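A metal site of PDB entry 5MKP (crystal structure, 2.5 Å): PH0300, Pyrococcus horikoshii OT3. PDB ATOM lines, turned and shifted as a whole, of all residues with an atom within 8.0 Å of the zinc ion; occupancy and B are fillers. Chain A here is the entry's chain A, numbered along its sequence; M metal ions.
O of Cys 290 lies within hydrogen-bond range of N of Leu 295, 3.1 Å away.
The side-chain hydroxyl (OG) of Ser 282 is in hydrogen-bond range of the backbone NH (N) of Cys 287, at 3.1 Å.
The side-chain hydroxyl of Tyr 140 sits close to the side-chain sulfur of Cys 278, at 3.2 Å.
The backbone NH (N) of Met 280 sits close to the side-chain sulfur (SG) of Cys 278 (3.5 Å).
SG of Cys 275 lies close to N of Ile 277, at 3.2 Å.
The backbone carbonyl oxygen (O) of Met 280 is in hydrogen-bond range of the backbone NH (N) of Cys 275 (2.8 Å).
Of the 21 residues printed, 4 come within 4 Å of the zinc ion.
The zinc ion is bound by the side-chain sulfur of Cys 290 (2.3 Å), the side-chain sulfur of Cys 278 (2.4 Å), the side-chain sulfur of Cys 275 (2.4 Å) and the side-chain sulfur of Cys 287 (2.6 Å).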
ATOM      1  N   TYR A 140      31.582  -1.445   3.102  1.00  0.00           N
ATOM      2  CA  TYR A 140      30.679  -0.327   2.893  1.00  0.00           C
ATOM      3  C   TYR A 140      31.171   0.566   1.743  1.00  0.00           C
ATOM      4  O   TYR A 140      30.363   0.942   0.887  1.00  0.00           O
ATOM      5  CB  TYR A 140      30.530   0.495   4.191  1.00  0.00           C
ATOM      6  CG  TYR A 140      29.718   1.749   3.975  1.00  0.00           C
ATOM      7  CD1 TYR A 140      30.319   2.935   3.551  1.00  0.00           C
ATOM      8  CD2 TYR A 140      28.334   1.730   4.089  1.00  0.00           C
ATOM      9  CE1 TYR A 140      29.564   4.067   3.270  1.00  0.00           C
ATOM     10  CE2 TYR A 140      27.568   2.877   3.845  1.00  0.00           C
ATOM     11  CZ  TYR A 140      28.192   4.040   3.447  1.00  0.00           C
ATOM     12  OH  TYR A 140      27.450   5.170   3.222  1.00  0.00           O
ATOM     13  N   LYS A 144      29.286   1.282  -1.685  1.00  0.00           N
ATOM     14  CA  LYS A 144      28.879   2.654  -1.968  1.00  0.00           C
ATOM     15  C   LYS A 144      29.633   3.262  -3.153  1.00  0.00           C
ATOM     16  O   LYS A 144      29.002   3.924  -3.973  1.00  0.00           O
ATOM     17  CB  LYS A 144      28.915   3.555  -0.731  1.00  0.00           C
ATOM     18  CG  LYS A 144      28.028   4.752  -0.934  1.00  0.00           C
ATOM     19  CD  LYS A 144      27.997   5.700   0.206  1.00  0.00           C
ATOM     20  CE  LYS A 144      26.675   6.466   0.195  1.00  0.00           C
ATOM     21  NZ  LYS A 144      26.650   7.524  -0.845  1.00  0.00           N
ATOM     22  N   GLU A 274      16.469   1.470   4.669  1.00  0.00           N
ATOM     23  CA  GLU A 274      17.448   2.445   4.167  1.00  0.00           C
ATOM     24  C   GLU A 274      17.931   3.315   5.312  1.00  0.00           C
ATOM     25  O   GLU A 274      17.106   3.782   6.094  1.00  0.00           O
ATOM     26  CB  GLU A 274      16.832   3.355   3.095  1.00  0.00           C
ATOM     27  CG  GLU A 274      17.193   2.972   1.666  1.00  0.00           C
ATOM     28  CD  GLU A 274      16.628   3.898   0.606  1.00  0.00           C
ATOM     29  OE1 GLU A 274      16.171   5.020   0.943  1.00  0.00           O
ATOM     30  OE2 GLU A 274      16.643   3.489  -0.581  1.00  0.00           O
ATOM     31  N   CYS A 275      19.241   3.555   5.386  1.00  0.00           N
ATOM     32  CA  CYS A 275      19.850   4.394   6.413  1.00  0.00           C
ATOM     33  C   CYS A 275      19.306   5.801   6.329  1.00  0.00           C
ATOM     34  O   CYS A 275      19.025   6.287   5.240  1.00  0.00           O
ATOM     35  CB  CYS A 275      21.378   4.371   6.312  1.00  0.00           C
ATOM     36  SG  CYS A 275      22.214   5.590   7.362  1.00  0.00           S
ATOM     37  N   LYS A 276      19.125   6.450   7.482  1.00  0.00           N
ATOM     38  CA  LYS A 276      18.585   7.805   7.542  1.00  0.00           C
ATOM     39  C   LYS A 276      19.640   8.864   7.254  1.00  0.00           C
ATOM     40  O   LYS A 276      19.295  10.026   7.006  1.00  0.00           O
ATOM     41  CB  LYS A 276      17.832   8.037   8.851  1.00  0.00           C
ATOM     42  CG  LYS A 276      16.478   7.330   8.860  1.00  0.00           C
ATOM     43  CD  LYS A 276      15.818   7.292  10.228  1.00  0.00           C
ATOM     44  CE  LYS A 276      14.459   6.635  10.170  1.00  0.00           C
ATOM     45  NZ  LYS A 276      13.851   6.477  11.513  1.00  0.00           N
ATOM     46  N   ILE A 277      20.929   8.469   7.229  1.00  0.00           N
ATOM     47  CA  ILE A 277      22.064   9.351   6.928  1.00  0.00           C
ATOM     48  C   ILE A 277      22.475   9.196   5.452  1.00  0.00           C
ATOM     49  O   ILE A 277      22.357  10.148   4.687  1.00  0.00           O
ATOM     50  CB  ILE A 277      23.264   9.130   7.921  1.00  0.00           C
ATOM     51  CG1 ILE A 277      22.866   9.351   9.416  1.00  0.00           C
ATOM     52  CG2 ILE A 277      24.504   9.967   7.539  1.00  0.00           C
ATOM     53  CD1 ILE A 277      22.282  10.763   9.812  1.00  0.00           C
ATOM     54  N   CYS A 278      22.952   8.002   5.058  1.00  0.00           N
ATOM     55  CA  CYS A 278      23.472   7.725   3.719  1.00  0.00           C
ATOM     56  C   CYS A 278      22.497   7.068   2.760  1.00  0.00           C
ATOM     57  O   CYS A 278      22.850   6.928   1.580  1.00  0.00           O
ATOM     58  CB  CYS A 278      24.753   6.907   3.824  1.00  0.00           C
ATOM     59  SG  CYS A 278      24.490   5.199   4.376  1.00  0.00           S
ATOM     60  N   ARG A 279      21.320   6.593   3.242  1.00  0.00           N
ATOM     61  CA  ARG A 279      20.314   5.905   2.437  1.00  0.00           C
ATOM     62  C   ARG A 279      20.799   4.532   1.903  1.00  0.00           C
ATOM     63  O   ARG A 279      20.248   4.015   0.926  1.00  0.00           O
ATOM     64  CB  ARG A 279      19.753   6.797   1.309  1.00  0.00           C
ATOM     65  CG  ARG A 279      18.518   7.589   1.706  1.00  0.00           C
ATOM     66  CD  ARG A 279      18.061   8.520   0.596  1.00  0.00           C
ATOM     67  NE  ARG A 279      18.740   9.822   0.628  1.00  0.00           N
ATOM     68  CZ  ARG A 279      19.711  10.196  -0.196  1.00  0.00           C
ATOM     69  NH1 ARG A 279      20.124   9.381  -1.152  1.00  0.00           N
ATOM     70  NH2 ARG A 279      20.258  11.399  -0.079  1.00  0.00           N
ATOM     71  N   MET A 280      21.813   3.936   2.565  1.00  0.00           N
ATOM     72  CA  MET A 280      22.347   2.620   2.213  1.00  0.00           C
ATOM     73  C   MET A 280      21.673   1.529   3.067  1.00  0.00           C
ATOM     74  O   MET A 280      21.113   1.872   4.115  1.00  0.00           O
ATOM     75  CB  MET A 280      23.889   2.584   2.320  1.00  0.00           C
ATOM     76  CG  MET A 280      24.615   3.443   1.278  1.00  0.00           C
ATOM     77  SD  MET A 280      24.116   3.256  -0.476  1.00  0.00           S
ATOM     78  CE  MET A 280      24.907   1.721  -0.874  1.00  0.00           C
ATOM     79  N   PRO A 281      21.665   0.238   2.643  1.00  0.00           N
ATOM     80  CA  PRO A 281      20.976  -0.804   3.441  1.00  0.00           C
ATOM     81  C   PRO A 281      21.344  -0.852   4.918  1.00  0.00           C
ATOM     82  O   PRO A 281      22.497  -1.059   5.293  1.00  0.00           O
ATOM     83  CB  PRO A 281      21.304  -2.101   2.705  1.00  0.00           C
ATOM     84  CG  PRO A 281      21.611  -1.704   1.320  1.00  0.00           C
ATOM     85  CD  PRO A 281      22.252  -0.351   1.414  1.00  0.00           C
ATOM     86  N   SER A 282      20.336  -0.632   5.751  1.00  0.00           N
ATOM     87  CA  SER A 282      20.440  -0.580   7.195  1.00  0.00           C
ATOM     88  C   SER A 282      19.442  -1.562   7.834  1.00  0.00           C
ATOM     89  O   SER A 282      18.311  -1.679   7.346  1.00  0.00           O
ATOM     90  CB  SER A 282      20.107   0.840   7.660  1.00  0.00           C
ATOM     91  OG  SER A 282      20.155   0.978   9.072  1.00  0.00           O
ATOM     92  N   ASP A 285      17.661   2.119  12.170  1.00  0.00           N
ATOM     93  CA  ASP A 285      17.324   3.434  11.627  1.00  0.00           C
ATOM     94  C   ASP A 285      18.512   4.060  10.887  1.00  0.00           C
ATOM     95  O   ASP A 285      18.316   4.695   9.841  1.00  0.00           O
ATOM     96  CB  ASP A 285      16.812   4.366  12.741  1.00  0.00           C
ATOM     97  CG  ASP A 285      15.391   4.086  13.199  1.00  0.00           C
ATOM     98  OD1 ASP A 285      14.810   3.057  12.754  1.00  0.00           O
ATOM     99  OD2 ASP A 285      14.836   4.903  13.973  1.00  0.00           O
ATOM    100  N   ILE A 286      19.730   3.846  11.419  1.00  0.00           N
ATOM    101  CA  ILE A 286      21.022   4.284  10.892  1.00  0.00           C
ATOM    102  C   ILE A 286      21.885   3.025  10.725  1.00  0.00           C
ATOM    103  O   ILE A 286      21.878   2.168  11.609  1.00  0.00           O
ATOM    104  CB  ILE A 286      21.666   5.356  11.834  1.00  0.00           C
ATOM    105  CG1 ILE A 286      20.818   6.645  11.869  1.00  0.00           C
ATOM    106  CG2 ILE A 286      23.126   5.660  11.434  1.00  0.00           C
ATOM    107  CD1 ILE A 286      20.830   7.372  13.164  1.00  0.00           C
ATOM    108  N   CYS A 287      22.593   2.897   9.589  1.00  0.00           N
ATOM    109  CA  CYS A 287      23.407   1.703   9.359  1.00  0.00           C
ATOM    110  C   CYS A 287      24.653   1.664  10.239  1.00  0.00           C
ATOM    111  O   CYS A 287      25.069   2.689  10.787  1.00  0.00           O
ATOM    112  CB  CYS A 287      23.743   1.516   7.878  1.00  0.00           C
ATOM    113  SG  CYS A 287      25.097   2.542   7.257  1.00  0.00           S
ATOM    114  N   ALA A 288      25.196   0.447  10.406  1.00  0.00           N
ATOM    115  CA  ALA A 288      26.357   0.133  11.215  1.00  0.00           C
ATOM    116  C   ALA A 288      27.569   1.031  10.893  1.00  0.00           C
ATOM    117  O   ALA A 288      28.145   1.586  11.827  1.00  0.00           O
ATOM    118  CB  ALA A 288      26.713  -1.343  11.071  1.00  0.00           C
ATOM    119  N   PHE A 289      27.902   1.228   9.597  1.00  0.00           N
ATOM    120  CA  PHE A 289      29.009   2.103   9.175  1.00  0.00           C
ATOM    121  C   PHE A 289      28.841   3.517   9.742  1.00  0.00           C
ATOM    122  O   PHE A 289      29.738   4.014  10.423  1.00  0.00           O
ATOM    123  CB  PHE A 289      29.135   2.134   7.643  1.00  0.00           C
ATOM    124  CG  PHE A 289      30.237   3.022   7.109  1.00  0.00           C
ATOM    125  CD1 PHE A 289      31.538   2.540   6.958  1.00  0.00           C
ATOM    126  CD2 PHE A 289      29.979   4.350   6.744  1.00  0.00           C
ATOM    127  CE1 PHE A 289      32.548   3.359   6.450  1.00  0.00           C
ATOM    128  CE2 PHE A 289      31.006   5.170   6.268  1.00  0.00           C
ATOM    129  CZ  PHE A 289      32.282   4.672   6.124  1.00  0.00           C
ATOM    130  N   CYS A 290      27.675   4.154   9.455  1.00  0.00           N
ATOM    131  CA  CYS A 290      27.304   5.482   9.898  1.00  0.00           C
ATOM    132  C   CYS A 290      27.267   5.613  11.404  1.00  0.00           C
ATOM    133  O   CYS A 290      27.707   6.632  11.927  1.00  0.00           O
ATOM    134  CB  CYS A 290      25.981   5.916   9.288  1.00  0.00           C
ATOM    135  SG  CYS A 290      26.088   6.352   7.551  1.00  0.00           S
ATOM    136  N   LYS A 291      26.701   4.581  12.093  1.00  0.00           N
ATOM    137  CA  LYS A 291      26.585   4.557  13.553  1.00  0.00           C
ATOM    138  C   LYS A 291      27.965   4.523  14.187  1.00  0.00           C
ATOM    139  O   LYS A 291      28.216   5.312  15.096  1.00  0.00           O
ATOM    140  CB  LYS A 291      25.720   3.384  14.031  1.00  0.00           C
ATOM    141  CG  LYS A 291      24.326   3.802  14.495  1.00  0.00           C
ATOM    142  CD  LYS A 291      23.717   2.779  15.464  1.00  0.00           C
ATOM    143  CE  LYS A 291      22.714   3.419  16.406  1.00  0.00           C
ATOM    144  NZ  LYS A 291      22.284   2.491  17.488  1.00  0.00           N
ATOM    145  N   LEU A 295      28.675   9.600  11.767  1.00  0.00           N
ATOM    146  CA  LEU A 295      28.425  10.486  10.628  1.00  0.00           C
ATOM    147  C   LEU A 295      26.978  10.957  10.559  1.00  0.00           C
ATOM    148  O   LEU A 295      26.043  10.169  10.695  1.00  0.00           O
ATOM    149  CB  LEU A 295      28.864   9.826   9.301  1.00  0.00           C
ATOM    150  CG  LEU A 295      30.295   9.272   9.240  1.00  0.00           C
ATOM    151  CD1 LEU A 295      30.459   8.354   8.051  1.00  0.00           C
ATOM    152  CD2 LEU A 295      31.340  10.371   9.240  1.00  0.00           C
ATOM    153  N   LYS A 297      26.310  13.105   7.908  1.00  0.00           N
ATOM    154  CA  LYS A 297      26.313  13.459   6.492  1.00  0.00           C
ATOM    155  C   LYS A 297      26.756  12.293   5.615  1.00  0.00           C
ATOM    156  O   LYS A 297      27.621  11.504   6.006  1.00  0.00           O
ATOM    157  CB  LYS A 297      27.202  14.694   6.221  1.00  0.00           C
ATOM    158  CG  LYS A 297      26.605  16.007   6.730  1.00  0.00           C
ATOM    159  CD  LYS A 297      27.546  17.179   6.498  1.00  0.00           C
ATOM    160  CE  LYS A 297      27.069  18.419   7.215  1.00  0.00           C
ATOM    161  NZ  LYS A 297      28.047  19.530   7.074  1.00  0.00           N
ATOM    162  N   GLU A 298      26.165  12.195   4.427  1.00  0.00           N
ATOM    163  CA  GLU A 298      26.460  11.158   3.437  1.00  0.00           C
ATOM    164  C   GLU A 298      27.816  11.435   2.759  1.00  0.00           C
ATOM    165  O   GLU A 298      28.200  12.595   2.595  1.00  0.00           O
ATOM    166  CB  GLU A 298      25.330  11.127   2.377  1.00  0.00           C
ATOM    167  CG  GLU A 298      25.345   9.931   1.435  1.00  0.00           C
ATOM    168  CD  GLU A 298      24.477  10.070   0.197  1.00  0.00           C
ATOM    169  OE1 GLU A 298      24.985   9.769  -0.909  1.00  0.00           O
ATOM    170  OE2 GLU A 298      23.296  10.458   0.324  1.00  0.00           O
HETATM  171 ZN    ZN M   1      24.438   4.960   6.716  1.00  0.00          ZN
